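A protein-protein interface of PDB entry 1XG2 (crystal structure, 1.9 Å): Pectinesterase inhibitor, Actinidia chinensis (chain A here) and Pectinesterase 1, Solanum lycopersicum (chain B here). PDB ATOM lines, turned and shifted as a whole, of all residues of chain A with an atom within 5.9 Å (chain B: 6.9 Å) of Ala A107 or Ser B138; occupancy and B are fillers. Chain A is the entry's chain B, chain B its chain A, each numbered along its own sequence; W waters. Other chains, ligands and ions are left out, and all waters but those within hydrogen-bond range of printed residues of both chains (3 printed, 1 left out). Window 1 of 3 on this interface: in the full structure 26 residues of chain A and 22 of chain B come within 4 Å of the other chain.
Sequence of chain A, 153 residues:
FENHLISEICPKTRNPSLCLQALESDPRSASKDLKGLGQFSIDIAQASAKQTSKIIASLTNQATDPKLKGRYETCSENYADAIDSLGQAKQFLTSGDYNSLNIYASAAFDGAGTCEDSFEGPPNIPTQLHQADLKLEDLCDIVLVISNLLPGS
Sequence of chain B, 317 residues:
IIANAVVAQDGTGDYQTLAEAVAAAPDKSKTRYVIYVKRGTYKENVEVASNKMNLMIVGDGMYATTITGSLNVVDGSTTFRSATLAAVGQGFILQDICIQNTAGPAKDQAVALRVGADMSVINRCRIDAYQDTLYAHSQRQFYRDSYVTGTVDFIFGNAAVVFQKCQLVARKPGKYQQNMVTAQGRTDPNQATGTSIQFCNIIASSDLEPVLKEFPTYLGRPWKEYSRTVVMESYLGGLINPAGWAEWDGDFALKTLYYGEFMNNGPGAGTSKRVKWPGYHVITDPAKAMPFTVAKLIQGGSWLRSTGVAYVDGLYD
The side-chain carboxylate of Asp B118 lies within hydrogen-bond range of the side-chain hydroxyl of Tyr A104, 2.7 Å away. The side-chain amide nitrogen of Gln B139 sits at hydrogen-bond distance from the side-chain hydroxyl of Ser A85, 3.2 Å away. The side-chain amide nitrogen (ND2) of Asn B158 lies within hydrogen-bond range of the side-chain carboxylate (OD2) of Asp A110, at 2.6 Å. NE2 of Gln B191 is in hydrogen-bond range of O of Ser A106 (3.2 Å). NE2 of Gln B191 lies within hydrogen-bond range of OD1 of Asp A110.
NH2 of Arg B140 is in salt-bridge range of OD2 of Asp B118 (2.9 Å). The backbone NH (N) of Asn B158 is in hydrogen-bond range of the backbone carbonyl oxygen (O) of Ala B136, 3.2 Å away. OG of Ser B138 is in hydrogen-bond range of ND1 of His B137 (2.8 Å). The side-chain amide nitrogen of Asn B158 sits close to the side-chain amide nitrogen of Gln B191 (3.2 Å). The side-chain hydroxyl of Thr B193 lies within hydrogen-bond range of the side-chain amide oxygen of Asn B158, 2.7 Å away. The backbone carbonyl oxygen (O) of Asn A102 sits at hydrogen-bond distance from the side-chain hydroxyl (OG) of Ser A106 (3.0 Å).
Asn A102 touches Gln B191 (OD1 to C, 3.7 Å). Gln B139 touches Ile A103. CG1 of Ile A103 touches CD of Arg B140, 3.9 Å away. Ala B160 touches Ile A103 (CB to CD1, 3.8 Å). Gln B139 touches Tyr A104 (OE1 to CD1, 3.8 Å). Ser B138 touches Ala A107. Ala A107 touches Gln B139. NE2 of Gln B191 touches CD2 of Phe A109, 3.7 Å away.
Printed residues of chain B within 4 Å of Ser A85: Gln B139. Printed residues of chain B within 4 Å of Ser A106: Gln B191. Ala A107 touches two residues of chain B. Ser B138 touches one residue of chain A. The nearest residue of chain B that does not touch Ala A107 is His B137 (5.0 Å).
Of the 13 printed residues of chain A, 8 touch a printed residue of chain B. Hydrophobic or aromatic side chains of chain A within 4 Å of the printed part of chain B: Ile A103, Tyr A104, Ala A107 and Phe A109. Hydrophobic or aromatic side chains of chain B that line the printed part of chain A: Ala B160. Among the printed residues, no Asp or Glu carboxylate lies within 4 Å of a Lys or Arg side-chain nitrogen of the other chain.
Water W3 lies within hydrogen-bond range of the side-chain carboxylate of Asp A110 (2.6 Å), the side-chain amide oxygen of Gln B191 (3.1 Å) and the side-chain amide nitrogen of Asn B158 (3.1 Å). Water W1 lies within hydrogen-bond range of O of Asn B158 (2.8 Å) and OD2 of Asp A110 (2.8 Å). Water W2 lies within hydrogen-bond range of O of Ile A103 (2.8 Å) and N of Gln B139 (2.9 Å).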
ATOM      1  N   ALA A  82      18.461 -29.695  24.329  1.00  0.00           N
ATOM      2  CA  ALA A  82      19.003 -30.010  23.004  1.00  0.00           C
ATOM      3  C   ALA A  82      20.046 -31.124  23.062  1.00  0.00           C
ATOM      4  O   ALA A  82      20.046 -32.030  22.214  1.00  0.00           O
ATOM      5  CB  ALA A  82      19.594 -28.770  22.358  1.00  0.00           C
ATOM      6  N   SER A  85      18.266 -34.370  23.658  1.00  0.00           N
ATOM      7  CA  SER A  85      17.517 -34.792  22.491  1.00  0.00           C
ATOM      8  C   SER A  85      18.429 -35.349  21.411  1.00  0.00           C
ATOM      9  O   SER A  85      18.077 -36.319  20.748  1.00  0.00           O
ATOM     10  CB  SER A  85      16.645 -33.654  21.933  1.00  0.00           C
ATOM     11  OG  SER A  85      15.527 -33.427  22.782  1.00  0.00           O
ATOM     12  N   ASN A 102      13.752 -37.273  13.309  1.00  0.00           N
ATOM     13  CA  ASN A 102      13.421 -35.920  12.845  1.00  0.00           C
ATOM     14  C   ASN A 102      12.908 -35.051  14.005  1.00  0.00           C
ATOM     15  O   ASN A 102      13.431 -33.975  14.264  1.00  0.00           O
ATOM     16  CB  ASN A 102      12.414 -35.956  11.697  1.00  0.00           C
ATOM     17  CG  ASN A 102      12.190 -34.601  11.095  1.00  0.00           C
ATOM     18  OD1 ASN A 102      11.665 -33.672  11.745  1.00  0.00           O
ATOM     19  ND2 ASN A 102      12.568 -34.469   9.848  1.00  0.00           N
ATOM     20  N   ILE A 103      11.932 -35.566  14.740  1.00  0.00           N
ATOM     21  CA  ILE A 103      11.343 -34.853  15.870  1.00  0.00           C
ATOM     22  C   ILE A 103      12.404 -34.403  16.892  1.00  0.00           C
ATOM     23  O   ILE A 103      12.374 -33.253  17.356  1.00  0.00           O
ATOM     24  CB  ILE A 103      10.284 -35.748  16.552  1.00  0.00           C
ATOM     25  CG1 ILE A 103       9.111 -36.031  15.601  1.00  0.00           C
ATOM     26  CG2 ILE A 103       9.801 -35.116  17.869  1.00  0.00           C
ATOM     27  CD1 ILE A 103       8.316 -34.835  15.196  1.00  0.00           C
ATOM     28  N   TYR A 104      13.331 -35.288  17.242  1.00  0.00           N
ATOM     29  CA  TYR A 104      14.321 -34.953  18.256  1.00  0.00           C
ATOM     30  C   TYR A 104      15.367 -33.977  17.713  1.00  0.00           C
ATOM     31  O   TYR A 104      15.777 -33.074  18.436  1.00  0.00           O
ATOM     32  CB  TYR A 104      14.972 -36.192  18.860  1.00  0.00           C
ATOM     33  CG  TYR A 104      14.088 -36.859  19.892  1.00  0.00           C
ATOM     34  CD1 TYR A 104      12.857 -37.394  19.522  1.00  0.00           C
ATOM     35  CD2 TYR A 104      14.450 -36.919  21.238  1.00  0.00           C
ATOM     36  CE1 TYR A 104      12.033 -38.008  20.447  1.00  0.00           C
ATOM     37  CE2 TYR A 104      13.602 -37.551  22.190  1.00  0.00           C
ATOM     38  CZ  TYR A 104      12.404 -38.093  21.762  1.00  0.00           C
ATOM     39  OH  TYR A 104      11.534 -38.705  22.644  1.00  0.00           O
ATOM     40  N   ALA A 105      15.766 -34.131  16.452  1.00  0.00           N
ATOM     41  CA  ALA A 105      16.646 -33.139  15.825  1.00  0.00           C
ATOM     42  C   ALA A 105      15.952 -31.790  15.662  1.00  0.00           C
ATOM     43  O   ALA A 105      16.595 -30.747  15.807  1.00  0.00           O
ATOM     44  CB  ALA A 105      17.203 -33.637  14.481  1.00  0.00           C
ATOM     45  N   SER A 106      14.643 -31.800  15.396  1.00  0.00           N
ATOM     46  CA  SER A 106      13.865 -30.570  15.314  1.00  0.00           C
ATOM     47  C   SER A 106      13.821 -29.864  16.664  1.00  0.00           C
ATOM     48  O   SER A 106      13.933 -28.635  16.732  1.00  0.00           O
ATOM     49  CB  SER A 106      12.432 -30.841  14.833  1.00  0.00           C
ATOM     50  OG  SER A 106      12.400 -31.227  13.479  1.00  0.00           O
ATOM     51  N   ALA A 107      13.685 -30.643  17.742  1.00  0.00           N
ATOM     52  CA  ALA A 107      13.648 -30.081  19.090  1.00  0.00           C
ATOM     53  C   ALA A 107      14.994 -29.467  19.465  1.00  0.00           C
ATOM     54  O   ALA A 107      15.049 -28.390  20.072  1.00  0.00           O
ATOM     55  CB  ALA A 107      13.247 -31.150  20.129  1.00  0.00           C
ATOM     56  N   ALA A 108      16.075 -30.141  19.093  1.00  0.00           N
ATOM     57  CA  ALA A 108      17.427 -29.649  19.355  1.00  0.00           C
ATOM     58  C   ALA A 108      17.667 -28.327  18.636  1.00  0.00           C
ATOM     59  O   ALA A 108      18.106 -27.364  19.244  1.00  0.00           O
ATOM     60  CB  ALA A 108      18.457 -30.670  18.908  1.00  0.00           C
ATOM     61  N   PHE A 109      17.369 -28.302  17.344  1.00  0.00           N
ATOM     62  CA  PHE A 109      17.392 -27.080  16.537  1.00  0.00           C
ATOM     63  C   PHE A 109      16.708 -25.933  17.255  1.00  0.00           C
ATOM     64  O   PHE A 109      17.219 -24.826  17.307  1.00  0.00           O
ATOM     65  CB  PHE A 109      16.698 -27.369  15.192  1.00  0.00           C
ATOM     66  CG  PHE A 109      16.653 -26.205  14.247  1.00  0.00           C
ATOM     67  CD1 PHE A 109      17.427 -26.204  13.104  1.00  0.00           C
ATOM     68  CD2 PHE A 109      15.816 -25.124  14.482  1.00  0.00           C
ATOM     69  CE1 PHE A 109      17.389 -25.130  12.222  1.00  0.00           C
ATOM     70  CE2 PHE A 109      15.766 -24.053  13.603  1.00  0.00           C
ATOM     71  CZ  PHE A 109      16.554 -24.059  12.472  1.00  0.00           C
ATOM     72  N   ASP A 110      15.531 -26.206  17.799  1.00  0.00           N
ATOM     73  CA  ASP A 110      14.710 -25.191  18.451  1.00  0.00           C
ATOM     74  C   ASP A 110      15.225 -24.740  19.820  1.00  0.00           C
ATOM     75  O   ASP A 110      14.767 -23.730  20.346  1.00  0.00           O
ATOM     76  CB  ASP A 110      13.285 -25.715  18.624  1.00  0.00           C
ATOM     77  CG  ASP A 110      12.492 -25.700  17.332  1.00  0.00           C
ATOM     78  OD1 ASP A 110      12.926 -25.074  16.328  1.00  0.00           O
ATOM     79  OD2 ASP A 110      11.388 -26.265  17.246  1.00  0.00           O
ATOM     80  N   GLY A 111      16.116 -25.499  20.434  1.00  0.00           N
ATOM     81  CA  GLY A 111      16.800 -25.019  21.624  1.00  0.00           C
ATOM     82  C   GLY A 111      17.593 -23.752  21.325  1.00  0.00           C
ATOM     83  O   GLY A 111      17.537 -22.769  22.071  1.00  0.00           O
ATOM     84  N   ALA A 112      18.325 -23.769  20.215  1.00  0.00           N
ATOM     85  CA  ALA A 112      19.109 -22.605  19.794  1.00  0.00           C
ATOM     86  C   ALA A 112      18.180 -21.455  19.395  1.00  0.00           C
ATOM     87  O   ALA A 112      18.433 -20.294  19.711  1.00  0.00           O
ATOM     88  CB  ALA A 112      20.014 -22.980  18.637  1.00  0.00           C
ATOM     89  N   ALA B  87       6.881 -28.928  31.326  1.00  0.00           N
ATOM     90  CA  ALA B  87       7.192 -30.356  31.348  1.00  0.00           C
ATOM     91  C   ALA B  87       7.952 -30.774  30.096  1.00  0.00           C
ATOM     92  O   ALA B  87       7.527 -30.493  28.985  1.00  0.00           O
ATOM     93  CB  ALA B  87       5.924 -31.166  31.470  1.00  0.00           C
ATOM     94  N   VAL B  88       9.078 -31.448  30.294  1.00  0.00           N
ATOM     95  CA  VAL B  88       9.864 -31.977  29.192  1.00  0.00           C
ATOM     96  C   VAL B  88      10.151 -33.464  29.346  1.00  0.00           C
ATOM     97  O   VAL B  88      10.663 -34.073  28.426  1.00  0.00           O
ATOM     98  CB  VAL B  88      11.177 -31.191  28.988  1.00  0.00           C
ATOM     99  CG1 VAL B  88      10.864 -29.718  28.705  1.00  0.00           C
ATOM    100  CG2 VAL B  88      12.102 -31.316  30.182  1.00  0.00           C
ATOM    101  N   VAL B 115       4.964 -27.318  27.208  1.00  0.00           N
ATOM    102  CA  VAL B 115       5.306 -28.714  27.022  1.00  0.00           C
ATOM    103  C   VAL B 115       6.389 -28.847  25.960  1.00  0.00           C
ATOM    104  O   VAL B 115       6.230 -28.357  24.848  1.00  0.00           O
ATOM    105  CB  VAL B 115       4.073 -29.521  26.627  1.00  0.00           C
ATOM    106  CG1 VAL B 115       4.419 -30.987  26.495  1.00  0.00           C
ATOM    107  CG2 VAL B 115       2.943 -29.323  27.670  1.00  0.00           C
ATOM    108  N   GLY B 116       7.487 -29.502  26.335  1.00  0.00           N
ATOM    109  CA  GLY B 116       8.540 -29.944  25.425  1.00  0.00           C
ATOM    110  C   GLY B 116       8.883 -31.411  25.677  1.00  0.00           C
ATOM    111  O   GLY B 116      10.034 -31.814  25.551  1.00  0.00           O
ATOM    112  N   ALA B 117       7.858 -32.197  26.015  1.00  0.00           N
ATOM    113  CA  ALA B 117       7.956 -33.601  26.353  1.00  0.00           C
ATOM    114  C   ALA B 117       7.402 -34.414  25.202  1.00  0.00           C
ATOM    115  O   ALA B 117       6.263 -34.215  24.769  1.00  0.00           O
ATOM    116  CB  ALA B 117       7.153 -33.904  27.621  1.00  0.00           C
ATOM    117  N   ASP B 118       8.210 -35.324  24.699  1.00  0.00           N
ATOM    118  CA  ASP B 118       7.783 -36.202  23.633  1.00  0.00           C
ATOM    119  C   ASP B 118       6.808 -37.256  24.139  1.00  0.00           C
ATOM    120  O   ASP B 118       6.935 -37.740  25.269  1.00  0.00           O
ATOM    121  CB  ASP B 118       8.991 -36.865  23.000  1.00  0.00           C
ATOM    122  CG  ASP B 118       8.647 -37.606  21.734  1.00  0.00           C
ATOM    123  OD1 ASP B 118       7.953 -37.041  20.875  1.00  0.00           O
ATOM    124  OD2 ASP B 118       9.057 -38.755  21.499  1.00  0.00           O
ATOM    125  N   SER B 120       3.684 -36.940  24.903  1.00  0.00           N
ATOM    126  CA  SER B 120       2.918 -36.403  26.015  1.00  0.00           C
ATOM    127  C   SER B 120       1.431 -36.293  25.668  1.00  0.00           C
ATOM    128  O   SER B 120       1.057 -36.072  24.510  1.00  0.00           O
ATOM    129  CB  SER B 120       3.482 -35.037  26.421  1.00  0.00           C
ATOM    130  OG  SER B 120       3.580 -34.189  25.286  1.00  0.00           O
ATOM    131  N   TYR B 135       2.337 -23.011  25.329  1.00  0.00           N
ATOM    132  CA  TYR B 135       3.598 -23.145  24.620  1.00  0.00           C
ATOM    133  C   TYR B 135       3.848 -24.622  24.341  1.00  0.00           C
ATOM    134  O   TYR B 135       4.505 -25.314  25.130  1.00  0.00           O
ATOM    135  CB  TYR B 135       4.730 -22.568  25.493  1.00  0.00           C
ATOM    136  CG  TYR B 135       5.995 -22.126  24.788  1.00  0.00           C
ATOM    137  CD1 TYR B 135       6.264 -22.457  23.469  1.00  0.00           C
ATOM    138  CD2 TYR B 135       6.919 -21.329  25.465  1.00  0.00           C
ATOM    139  CE1 TYR B 135       7.430 -22.024  22.840  1.00  0.00           C
ATOM    140  CE2 TYR B 135       8.070 -20.891  24.858  1.00  0.00           C
ATOM    141  CZ  TYR B 135       8.332 -21.233  23.554  1.00  0.00           C
ATOM    142  OH  TYR B 135       9.497 -20.773  22.985  1.00  0.00           O
ATOM    143  N   ALA B 136       3.283 -25.098  23.233  1.00  0.00           N
ATOM    144  CA  ALA B 136       3.537 -26.432  22.739  1.00  0.00           C
ATOM    145  C   ALA B 136       4.841 -26.324  21.974  1.00  0.00           C
ATOM    146  O   ALA B 136       4.851 -26.129  20.756  1.00  0.00           O
ATOM    147  CB  ALA B 136       2.397 -26.890  21.845  1.00  0.00           C
ATOM    148  N   HIS B 137       5.927 -26.428  22.737  1.00  0.00           N
ATOM    149  CA  HIS B 137       7.265 -25.986  22.353  1.00  0.00           C
ATOM    150  C   HIS B 137       7.907 -26.893  21.301  1.00  0.00           C
ATOM    151  O   HIS B 137       8.378 -26.434  20.259  1.00  0.00           O
ATOM    152  CB  HIS B 137       8.150 -25.898  23.606  1.00  0.00           C
ATOM    153  CG  HIS B 137       9.559 -25.483  23.330  1.00  0.00           C
ATOM    154  ND1 HIS B 137      10.473 -26.316  22.733  1.00  0.00           N
ATOM    155  CD2 HIS B 137      10.214 -24.325  23.576  1.00  0.00           C
ATOM    156  CE1 HIS B 137      11.622 -25.679  22.590  1.00  0.00           C
ATOM    157  NE2 HIS B 137      11.494 -24.468  23.097  1.00  0.00           N
ATOM    158  N   SER B 138       7.918 -28.185  21.582  1.00  0.00           N
ATOM    159  CA  SER B 138       8.633 -29.139  20.748  1.00  0.00           C
ATOM    160  C   SER B 138       8.186 -30.522  21.119  1.00  0.00           C
ATOM    161  O   SER B 138       7.479 -30.709  22.115  1.00  0.00           O
ATOM    162  CB  SER B 138      10.149 -29.000  20.933  1.00  0.00           C
ATOM    163  OG  SER B 138      10.501 -29.055  22.302  1.00  0.00           O
ATOM    164  N   GLN B 139       8.619 -31.483  20.313  1.00  0.00           N
ATOM    165  CA  GLN B 139       8.301 -32.904  20.459  1.00  0.00           C
ATOM    166  C   GLN B 139       6.846 -33.197  20.110  1.00  0.00           C
ATOM    167  O   GLN B 139       6.110 -32.310  19.675  1.00  0.00           O
ATOM    168  CB  GLN B 139       8.675 -33.466  21.848  1.00  0.00           C
ATOM    169  CG  GLN B 139      10.034 -33.056  22.408  1.00  0.00           C
ATOM    170  CD  GLN B 139      11.231 -33.738  21.738  1.00  0.00           C
ATOM    171  OE1 GLN B 139      11.142 -34.186  20.602  1.00  0.00           O
ATOM    172  NE2 GLN B 139      12.360 -33.777  22.438  1.00  0.00           N
ATOM    173  N   ARG B 140       6.453 -34.464  20.245  1.00  0.00           N
ATOM    174  CA  ARG B 140       5.122 -34.913  19.833  1.00  0.00           C
ATOM    175  C   ARG B 140       4.153 -34.874  21.012  1.00  0.00           C
ATOM    176  O   ARG B 140       4.424 -35.450  22.070  1.00  0.00           O
ATOM    177  CB  ARG B 140       5.162 -36.322  19.246  1.00  0.00           C
ATOM    178  CG  ARG B 140       5.835 -36.402  17.890  1.00  0.00           C
ATOM    179  CD  ARG B 140       6.206 -37.810  17.450  1.00  0.00           C
ATOM    180  NE  ARG B 140       7.214 -38.413  18.309  1.00  0.00           N
ATOM    181  CZ  ARG B 140       7.957 -39.492  18.005  1.00  0.00           C
ATOM    182  NH1 ARG B 140       7.824 -40.118  16.843  1.00  0.00           N
ATOM    183  NH2 ARG B 140       8.847 -39.928  18.871  1.00  0.00           N
ATOM    184  N   GLN B 141       3.015 -34.226  20.786  1.00  0.00           N
ATOM    185  CA  GLN B 141       2.031 -33.942  21.829  1.00  0.00           C
ATOM    186  C   GLN B 141       0.609 -34.194  21.315  1.00  0.00           C
ATOM    187  O   GLN B 141       0.307 -33.963  20.150  1.00  0.00           O
ATOM    188  CB  GLN B 141       2.158 -32.493  22.320  1.00  0.00           C
ATOM    189  CG  GLN B 141       3.588 -32.055  22.617  1.00  0.00           C
ATOM    190  CD  GLN B 141       3.728 -30.612  23.073  1.00  0.00           C
ATOM    191  OE1 GLN B 141       4.843 -30.067  23.067  1.00  0.00           O
ATOM    192  NE2 GLN B 141       2.639 -30.003  23.475  1.00  0.00           N
ATOM    193  N   PHE B 156       1.117 -21.765  20.626  1.00  0.00           N
ATOM    194  CA  PHE B 156       2.308 -21.378  19.879  1.00  0.00           C
ATOM    195  C   PHE B 156       3.486 -22.293  20.176  1.00  0.00           C
ATOM    196  O   PHE B 156       3.489 -22.996  21.179  1.00  0.00           O
ATOM    197  CB  PHE B 156       2.667 -19.911  20.168  1.00  0.00           C
ATOM    198  CG  PHE B 156       3.302 -19.693  21.506  1.00  0.00           C
ATOM    199  CD1 PHE B 156       4.658 -19.384  21.607  1.00  0.00           C
ATOM    200  CD2 PHE B 156       2.562 -19.805  22.662  1.00  0.00           C
ATOM    201  CE1 PHE B 156       5.261 -19.191  22.839  1.00  0.00           C
ATOM    202  CE2 PHE B 156       3.159 -19.603  23.899  1.00  0.00           C
ATOM    203  CZ  PHE B 156       4.511 -19.287  23.986  1.00  0.00           C
ATOM    204  N   GLY B 157       4.485 -22.265  19.296  1.00  0.00           N
ATOM    205  CA  GLY B 157       5.648 -23.132  19.417  1.00  0.00           C
ATOM    206  C   GLY B 157       5.876 -23.945  18.153  1.00  0.00           C
ATOM    207  O   GLY B 157       5.371 -23.604  17.087  1.00  0.00           O
ATOM    208  N   ASN B 158       6.609 -25.042  18.282  1.00  0.00           N
ATOM    209  CA  ASN B 158       6.976 -25.856  17.139  1.00  0.00           C
ATOM    210  C   ASN B 158       6.952 -27.341  17.464  1.00  0.00           C
ATOM    211  O   ASN B 158       7.770 -28.112  16.959  1.00  0.00           O
ATOM    212  CB  ASN B 158       8.350 -25.432  16.631  1.00  0.00           C
ATOM    213  CG  ASN B 158       8.685 -25.997  15.271  1.00  0.00           C
ATOM    214  OD1 ASN B 158       7.785 -26.172  14.420  1.00  0.00           O
ATOM    215  ND2 ASN B 158       9.952 -26.316  15.047  1.00  0.00           N
ATOM    216  N   ALA B 159       5.982 -27.744  18.288  1.00  0.00           N
ATOM    217  CA  ALA B 159       5.714 -29.173  18.503  1.00  0.00           C
ATOM    218  C   ALA B 159       5.165 -29.794  17.232  1.00  0.00           C
ATOM    219  O   ALA B 159       4.706 -29.091  16.346  1.00  0.00           O
ATOM    220  CB  ALA B 159       4.695 -29.364  19.630  1.00  0.00           C
ATOM    221  N   ALA B 160       5.226 -31.118  17.138  1.00  0.00           N
ATOM    222  CA  ALA B 160       4.307 -31.834  16.272  1.00  0.00           C
ATOM    223  C   ALA B 160       3.143 -32.179  17.196  1.00  0.00           C
ATOM    224  O   ALA B 160       3.295 -32.975  18.127  1.00  0.00           O
ATOM    225  CB  ALA B 160       4.940 -33.071  15.708  1.00  0.00           C
ATOM    226  N   GLN B 191      11.908 -29.767   9.141  1.00  0.00           N
ATOM    227  CA  GLN B 191      11.325 -30.161  10.413  1.00  0.00           C
ATOM    228  C   GLN B 191       9.921 -30.749  10.206  1.00  0.00           C
ATOM    229  O   GLN B 191       9.075 -30.124   9.574  1.00  0.00           O
ATOM    230  CB  GLN B 191      11.246 -28.964  11.379  1.00  0.00           C
ATOM    231  CG  GLN B 191      12.575 -28.373  11.849  1.00  0.00           C
ATOM    232  CD  GLN B 191      12.381 -27.159  12.772  1.00  0.00           C
ATOM    233  OE1 GLN B 191      11.797 -26.138  12.372  1.00  0.00           O
ATOM    234  NE2 GLN B 191      12.855 -27.271  13.996  1.00  0.00           N
ATOM    235  N   THR B 193       7.186 -30.877  11.870  1.00  0.00           N
ATOM    236  CA  THR B 193       6.403 -30.311  12.953  1.00  0.00           C
ATOM    237  C   THR B 193       5.246 -29.527  12.386  1.00  0.00           C
ATOM    238  O   THR B 193       5.174 -29.271  11.181  1.00  0.00           O
ATOM    239  CB  THR B 193       7.273 -29.399  13.796  1.00  0.00           C
ATOM    240  OG1 THR B 193       7.906 -28.433  12.949  1.00  0.00           O
ATOM    241  CG2 THR B 193       8.420 -30.172  14.421  1.00  0.00           C
HETATM  242  O   HOH W   1      10.404 -28.920  17.322  1.00  0.00           O
HETATM  243  O   HOH W   2      10.257 -31.486  17.967  1.00  0.00           O
HETATM  244  O   HOH W   3      11.715 -23.821  14.444  1.00  0.00           O
